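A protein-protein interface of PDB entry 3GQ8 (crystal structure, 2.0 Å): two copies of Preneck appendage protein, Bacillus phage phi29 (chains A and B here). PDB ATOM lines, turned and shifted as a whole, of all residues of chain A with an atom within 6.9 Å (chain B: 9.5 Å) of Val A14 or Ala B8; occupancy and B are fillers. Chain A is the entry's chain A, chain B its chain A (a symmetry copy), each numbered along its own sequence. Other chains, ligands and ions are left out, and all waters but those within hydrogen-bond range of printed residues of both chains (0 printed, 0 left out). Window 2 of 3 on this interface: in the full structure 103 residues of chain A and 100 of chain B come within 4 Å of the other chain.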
ATOM      1  N   ASP A   9     -18.096 -12.393  -4.117  1.00  0.00           N
ATOM      2  CA  ASP A   9     -18.441 -13.773  -3.791  1.00  0.00           C
ATOM      3  C   ASP A   9     -17.379 -14.777  -4.236  1.00  0.00           C
ATOM      4  O   ASP A   9     -17.156 -15.786  -3.558  1.00  0.00           O
ATOM      5  CB  ASP A   9     -19.809 -14.140  -4.365  1.00  0.00           C
ATOM      6  CG  ASP A   9     -20.959 -13.508  -3.592  1.00  0.00           C
ATOM      7  OD1 ASP A   9     -20.721 -12.597  -2.759  1.00  0.00           O
ATOM      8  OD2 ASP A   9     -22.114 -13.930  -3.817  1.00  0.00           O
ATOM      9  N   LEU A  10     -16.721 -14.502  -5.361  1.00  0.00           N
ATOM     10  CA  LEU A  10     -15.615 -15.345  -5.810  1.00  0.00           C
ATOM     11  C   LEU A  10     -14.404 -15.235  -4.888  1.00  0.00           C
ATOM     12  O   LEU A  10     -13.790 -16.244  -4.556  1.00  0.00           O
ATOM     13  CB  LEU A  10     -15.205 -15.029  -7.250  1.00  0.00           C
ATOM     14  CG  LEU A  10     -16.051 -15.631  -8.371  1.00  0.00           C
ATOM     15  CD1 LEU A  10     -15.357 -15.397  -9.702  1.00  0.00           C
ATOM     16  CD2 LEU A  10     -16.294 -17.128  -8.152  1.00  0.00           C
ATOM     17  N   VAL A  11     -14.059 -14.009  -4.499  1.00  0.00           N
ATOM     18  CA  VAL A  11     -12.968 -13.775  -3.545  1.00  0.00           C
ATOM     19  C   VAL A  11     -13.256 -14.491  -2.209  1.00  0.00           C
ATOM     20  O   VAL A  11     -12.423 -15.253  -1.718  1.00  0.00           O
ATOM     21  CB  VAL A  11     -12.702 -12.257  -3.344  1.00  0.00           C
ATOM     22  CG1 VAL A  11     -11.699 -12.012  -2.230  1.00  0.00           C
ATOM     23  CG2 VAL A  11     -12.207 -11.633  -4.644  1.00  0.00           C
ATOM     24  N   ILE A  12     -14.447 -14.263  -1.656  1.00  0.00           N
ATOM     25  CA  ILE A  12     -14.901 -14.936  -0.426  1.00  0.00           C
ATOM     26  C   ILE A  12     -14.779 -16.465  -0.509  1.00  0.00           C
ATOM     27  O   ILE A  12     -14.284 -17.097   0.432  1.00  0.00           O
ATOM     28  CB  ILE A  12     -16.342 -14.501  -0.028  1.00  0.00           C
ATOM     29  CG1 ILE A  12     -16.343 -13.036   0.420  1.00  0.00           C
ATOM     30  CG2 ILE A  12     -16.906 -15.387   1.088  1.00  0.00           C
ATOM     31  CD1 ILE A  12     -17.706 -12.385   0.405  1.00  0.00           C
ATOM     32  N   GLN A  13     -15.201 -17.051  -1.632  1.00  0.00           N
ATOM     33  CA  GLN A  13     -15.054 -18.498  -1.850  1.00  0.00           C
ATOM     34  C   GLN A  13     -13.615 -18.983  -1.728  1.00  0.00           C
ATOM     35  O   GLN A  13     -13.366 -20.065  -1.185  1.00  0.00           O
ATOM     36  CB  GLN A  13     -15.607 -18.915  -3.209  1.00  0.00           C
ATOM     37  CG  GLN A  13     -17.095 -19.172  -3.216  1.00  0.00           C
ATOM     38  CD  GLN A  13     -17.632 -19.447  -4.612  1.00  0.00           C
ATOM     39  OE1 GLN A  13     -16.906 -19.921  -5.496  1.00  0.00           O
ATOM     40  NE2 GLN A  13     -18.916 -19.145  -4.820  1.00  0.00           N
ATOM     41  N   VAL A  14     -12.675 -18.195  -2.247  1.00  0.00           N
ATOM     42  CA  VAL A  14     -11.251 -18.516  -2.141  1.00  0.00           C
ATOM     43  C   VAL A  14     -10.794 -18.459  -0.673  1.00  0.00           C
ATOM     44  O   VAL A  14     -10.087 -19.353  -0.202  1.00  0.00           O
ATOM     45  CB  VAL A  14     -10.375 -17.597  -3.044  1.00  0.00           C
ATOM     46  CG1 VAL A  14      -8.896 -17.868  -2.824  1.00  0.00           C
ATOM     47  CG2 VAL A  14     -10.724 -17.801  -4.513  1.00  0.00           C
ATOM     48  N   ILE A  15     -11.224 -17.418   0.039  1.00  0.00           N
ATOM     49  CA  ILE A  15     -10.895 -17.251   1.459  1.00  0.00           C
ATOM     50  C   ILE A  15     -11.451 -18.410   2.285  1.00  0.00           C
ATOM     51  O   ILE A  15     -10.721 -19.009   3.075  1.00  0.00           O
ATOM     52  CB  ILE A  15     -11.406 -15.901   2.027  1.00  0.00           C
ATOM     53  CG1 ILE A  15     -10.733 -14.729   1.318  1.00  0.00           C
ATOM     54  CG2 ILE A  15     -11.137 -15.802   3.530  1.00  0.00           C
ATOM     55  CD1 ILE A  15     -11.552 -13.448   1.349  1.00  0.00           C
ATOM     56  N   ASP A  16     -12.733 -18.716   2.089  1.00  0.00           N
ATOM     57  CA  ASP A  16     -13.392 -19.835   2.759  1.00  0.00           C
ATOM     58  C   ASP A  16     -12.620 -21.149   2.585  1.00  0.00           C
ATOM     59  O   ASP A  16     -12.454 -21.903   3.546  1.00  0.00           O
ATOM     60  CB  ASP A  16     -14.826 -20.010   2.241  1.00  0.00           C
ATOM     61  CG  ASP A  16     -15.744 -18.839   2.596  1.00  0.00           C
ATOM     62  OD1 ASP A  16     -15.324 -17.907   3.325  1.00  0.00           O
ATOM     63  OD2 ASP A  16     -16.907 -18.857   2.136  1.00  0.00           O
ATOM     64  N   GLU A  17     -12.158 -21.410   1.360  1.00  0.00           N
ATOM     65  CA  GLU A  17     -11.397 -22.620   1.028  1.00  0.00           C
ATOM     66  C   GLU A  17     -10.041 -22.708   1.707  1.00  0.00           C
ATOM     67  O   GLU A  17      -9.508 -23.810   1.883  1.00  0.00           O
ATOM     68  CB  GLU A  17     -11.173 -22.718  -0.477  1.00  0.00           C
ATOM     69  CG  GLU A  17     -12.199 -23.537  -1.209  1.00  0.00           C
ATOM     70  CD  GLU A  17     -11.770 -23.813  -2.643  1.00  0.00           C
ATOM     71  OE1 GLU A  17     -10.710 -24.458  -2.835  1.00  0.00           O
ATOM     72  OE2 GLU A  17     -12.494 -23.378  -3.576  1.00  0.00           O
ATOM     73  N   LEU A  18      -9.465 -21.555   2.047  1.00  0.00           N
ATOM     74  CA  LEU A  18      -8.192 -21.513   2.775  1.00  0.00           C
ATOM     75  C   LEU A  18      -8.314 -22.053   4.200  1.00  0.00           C
ATOM     76  O   LEU A  18      -7.330 -22.551   4.755  1.00  0.00           O
ATOM     77  CB  LEU A  18      -7.606 -20.096   2.814  1.00  0.00           C
ATOM     78  CG  LEU A  18      -6.632 -19.674   1.712  1.00  0.00           C
ATOM     79  CD1 LEU A  18      -6.173 -18.250   1.984  1.00  0.00           C
ATOM     80  CD2 LEU A  18      -5.431 -20.614   1.616  1.00  0.00           C
ATOM     81  N   LYS A  19      -9.509 -21.939   4.784  1.00  0.00           N
ATOM     82  CA  LYS A  19      -9.787 -22.491   6.113  1.00  0.00           C
ATOM     83  C   LYS A  19      -8.710 -22.087   7.121  1.00  0.00           C
ATOM     84  O   LYS A  19      -8.099 -22.947   7.768  1.00  0.00           O
ATOM     85  CB  LYS A  19      -9.880 -24.021   6.045  1.00  0.00           C
ATOM     86  CG  LYS A  19     -11.210 -24.544   5.564  1.00  0.00           C
ATOM     87  CD  LYS A  19     -11.116 -26.016   5.241  1.00  0.00           C
ATOM     88  CE  LYS A  19     -12.375 -26.477   4.520  1.00  0.00           C
ATOM     89  NZ  LYS A  19     -12.037 -27.356   3.359  1.00  0.00           N
ATOM     90  N   HIS B   6      -5.766 -19.886 -11.939  1.00  0.00           N
ATOM     91  CA  HIS B   6      -4.741 -18.825 -11.692  1.00  0.00           C
ATOM     92  C   HIS B   6      -5.336 -17.573 -11.043  1.00  0.00           C
ATOM     93  O   HIS B   6      -4.595 -16.731 -10.527  1.00  0.00           O
ATOM     94  CB  HIS B   6      -3.990 -18.449 -12.983  1.00  0.00           C
ATOM     95  CG  HIS B   6      -3.347 -19.613 -13.678  1.00  0.00           C
ATOM     96  ND1 HIS B   6      -2.346 -20.372 -13.099  1.00  0.00           N
ATOM     97  CD2 HIS B   6      -3.557 -20.143 -14.910  1.00  0.00           C
ATOM     98  CE1 HIS B   6      -1.974 -21.324 -13.940  1.00  0.00           C
ATOM     99  NE2 HIS B   6      -2.694 -21.207 -15.046  1.00  0.00           N
ATOM    100  N   PHE B   7      -6.664 -17.447 -11.077  1.00  0.00           N
ATOM    101  CA  PHE B   7      -7.350 -16.358 -10.371  1.00  0.00           C
ATOM    102  C   PHE B   7      -7.287 -16.567  -8.858  1.00  0.00           C
ATOM    103  O   PHE B   7      -6.974 -15.639  -8.116  1.00  0.00           O
ATOM    104  CB  PHE B   7      -8.807 -16.220 -10.829  1.00  0.00           C
ATOM    105  CG  PHE B   7      -9.673 -15.421  -9.884  1.00  0.00           C
ATOM    106  CD1 PHE B   7      -9.620 -14.030  -9.874  1.00  0.00           C
ATOM    107  CD2 PHE B   7     -10.541 -16.064  -9.004  1.00  0.00           C
ATOM    108  CE1 PHE B   7     -10.427 -13.285  -9.002  1.00  0.00           C
ATOM    109  CE2 PHE B   7     -11.346 -15.336  -8.125  1.00  0.00           C
ATOM    110  CZ  PHE B   7     -11.289 -13.940  -8.124  1.00  0.00           C
ATOM    111  N   ALA B   8      -7.596 -17.786  -8.420  1.00  0.00           N
ATOM    112  CA  ALA B   8      -7.551 -18.146  -7.004  1.00  0.00           C
ATOM    113  C   ALA B   8      -6.147 -17.964  -6.442  1.00  0.00           C
ATOM    114  O   ALA B   8      -5.984 -17.491  -5.321  1.00  0.00           O
ATOM    115  CB  ALA B   8      -8.039 -19.570  -6.790  1.00  0.00           C
ATOM    116  N   ASP B   9      -5.139 -18.321  -7.232  1.00  0.00           N
ATOM    117  CA  ASP B   9      -3.747 -18.122  -6.838  1.00  0.00           C
ATOM    118  C   ASP B   9      -3.376 -16.650  -6.676  1.00  0.00           C
ATOM    119  O   ASP B   9      -2.566 -16.305  -5.808  1.00  0.00           O
ATOM    120  CB  ASP B   9      -2.803 -18.815  -7.819  1.00  0.00           C
ATOM    121  CG  ASP B   9      -2.792 -20.329  -7.655  1.00  0.00           C
ATOM    122  OD1 ASP B   9      -3.677 -20.884  -6.956  1.00  0.00           O
ATOM    123  OD2 ASP B   9      -1.886 -20.972  -8.227  1.00  0.00           O
ATOM    124  N   LEU B  10      -3.967 -15.783  -7.497  1.00  0.00           N
ATOM    125  CA  LEU B  10      -3.760 -14.344  -7.347  1.00  0.00           C
ATOM    126  C   LEU B  10      -4.393 -13.806  -6.068  1.00  0.00           C
ATOM    127  O   LEU B  10      -3.779 -13.008  -5.366  1.00  0.00           O
ATOM    128  CB  LEU B  10      -4.282 -13.564  -8.556  1.00  0.00           C
ATOM    129  CG  LEU B  10      -3.395 -13.512  -9.799  1.00  0.00           C
ATOM    130  CD1 LEU B  10      -3.975 -12.514 -10.786  1.00  0.00           C
ATOM    131  CD2 LEU B  10      -1.952 -13.135  -9.445  1.00  0.00           C
ATOM    132  N   VAL B  11      -5.623 -14.232  -5.784  1.00  0.00           N
ATOM    133  CA  VAL B  11      -6.306 -13.858  -4.541  1.00  0.00           C
ATOM    134  C   VAL B  11      -5.492 -14.321  -3.315  1.00  0.00           C
ATOM    135  O   VAL B  11      -5.193 -13.522  -2.427  1.00  0.00           O
ATOM    136  CB  VAL B  11      -7.763 -14.399  -4.507  1.00  0.00           C
ATOM    137  CG1 VAL B  11      -8.410 -14.164  -3.152  1.00  0.00           C
ATOM    138  CG2 VAL B  11      -8.593 -13.743  -5.606  1.00  0.00           C
ATOM    139  N   ILE B  12      -5.114 -15.600  -3.301  1.00  0.00           N
ATOM    140  CA  ILE B  12      -4.263 -16.170  -2.241  1.00  0.00           C
ATOM    141  C   ILE B  12      -2.974 -15.365  -2.020  1.00  0.00           C
ATOM    142  O   ILE B  12      -2.615 -15.078  -0.871  1.00  0.00           O
ATOM    143  CB  ILE B  12      -3.956 -17.675  -2.496  1.00  0.00           C
ATOM    144  CG1 ILE B  12      -5.232 -18.507  -2.330  1.00  0.00           C
ATOM    145  CG2 ILE B  12      -2.869 -18.193  -1.548  1.00  0.00           C
ATOM    146  CD1 ILE B  12      -5.166 -19.875  -2.967  1.00  0.00           C
ATOM    147  N   GLN B  13      -2.300 -14.981  -3.106  1.00  0.00           N
ATOM    148  CA  GLN B  13      -1.100 -14.135  -3.010  1.00  0.00           C
ATOM    149  C   GLN B  13      -1.343 -12.823  -2.275  1.00  0.00           C
ATOM    150  O   GLN B  13      -0.486 -12.371  -1.507  1.00  0.00           O
ATOM    151  CB  GLN B  13      -0.521 -13.833  -4.389  1.00  0.00           C
ATOM    152  CG  GLN B  13       0.405 -14.903  -4.916  1.00  0.00           C
ATOM    153  CD  GLN B  13       0.848 -14.636  -6.346  1.00  0.00           C
ATOM    154  OE1 GLN B  13       0.895 -13.484  -6.798  1.00  0.00           O
ATOM    155  NE2 GLN B  13       1.178 -15.708  -7.072  1.00  0.00           N
ATOM    156  N   VAL B  14      -2.498 -12.209  -2.521  1.00  0.00           N
ATOM    157  CA  VAL B  14      -2.880 -10.974  -1.832  1.00  0.00           C
ATOM    158  C   VAL B  14      -3.093 -11.239  -0.331  1.00  0.00           C
ATOM    159  O   VAL B  14      -2.618 -10.474   0.513  1.00  0.00           O
ATOM    160  CB  VAL B  14      -4.134 -10.310  -2.473  1.00  0.00           C
ATOM    161  CG1 VAL B  14      -4.582  -9.100  -1.669  1.00  0.00           C
ATOM    162  CG2 VAL B  14      -3.844  -9.893  -3.910  1.00  0.00           C
ATOM    163  N   ILE B  15      -3.783 -12.334  -0.017  1.00  0.00           N
ATOM    164  CA  ILE B  15      -4.034 -12.730   1.374  1.00  0.00           C
ATOM    165  C   ILE B  15      -2.721 -13.001   2.106  1.00  0.00           C
ATOM    166  O   ILE B  15      -2.506 -12.479   3.201  1.00  0.00           O
ATOM    167  CB  ILE B  15      -4.964 -13.967   1.475  1.00  0.00           C
ATOM    168  CG1 ILE B  15      -6.340 -13.655   0.891  1.00  0.00           C
ATOM    169  CG2 ILE B  15      -5.125 -14.414   2.930  1.00  0.00           C
ATOM    170  CD1 ILE B  15      -7.083 -14.886   0.399  1.00  0.00           C
ATOM    171  N   ASP B  16      -1.855 -13.807   1.492  1.00  0.00           N
ATOM    172  CA  ASP B  16      -0.535 -14.116   2.037  1.00  0.00           C
ATOM    173  C   ASP B  16       0.255 -12.849   2.387  1.00  0.00           C
ATOM    174  O   ASP B  16       0.878 -12.779   3.449  1.00  0.00           O
ATOM    175  CB  ASP B  16       0.274 -14.969   1.051  1.00  0.00           C
ATOM    176  CG  ASP B  16      -0.315 -16.364   0.834  1.00  0.00           C
ATOM    177  OD1 ASP B  16      -1.308 -16.740   1.503  1.00  0.00           O
ATOM    178  OD2 ASP B  16       0.230 -17.094  -0.022  1.00  0.00           O
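CB of Leu A10 touches CE2 of Phe B7 (3.97 Å).
Val A14 touches Ala B8.
Val B11 touches Val A14 (CG1 to CG1, 3.8 Å).
Val A14 touches Ile B12 (CG1 to CG1, 3.8 Å).
CG1 of Ile A15 touches CD1 of Ile B15, at 3.8 Å.
CD1 of Leu A18 touches CD1 of Ile B15 (3.8 Å).
Val A14 touches Val B11, but with the chains exchanged Val A11 does not touch Val B14 (7.7 Å).
Val A14 touches Ile B12, but with the chains exchanged Ile A12 does not touch Val B14 (11.1 Å).
Ile A15 touches its own counterpart, Ile B15.
8 positions are printed for both chains.
Asp A9 touches none of the printed residues of chain B.
Printed residues of chain B within 4 Å of Val A14: Ala B8 (3.9 Å), Val B11 (3.8 Å) and Ile B12 (3.8 Å).
Of chain A, only Val A14 comes within 4 Å of Ala B8.
Printed residues of chain A within 4 Å of Val B11: Val A14.
Of the printed residues of chain A, Ile B12 touches Val A14 (3.8 Å).
The nearest residue of chain B that does not touch Val A14 is Phe B7 (4.4 Å).
Of the 11 printed residues of chain A, 4 touch a printed residue of chain B.
Printed residues of chain B that touch a printed residue of chain A: Phe B7, Ala B8, Val B11, Ile B12 and Ile B15.
Hydrophobic or aromatic side chains of chain B within 4 Å of the printed part of chain A: Phe B7, Ala B8, Val B11, Ile B12 and Ile B15.
Among the printed residues, 6 pairs touch across the chains.
Among the printed residues, no Asp or Glu carboxylate lies within 4 Å of a Lys or Arg side-chain nitrogen of the other chain.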
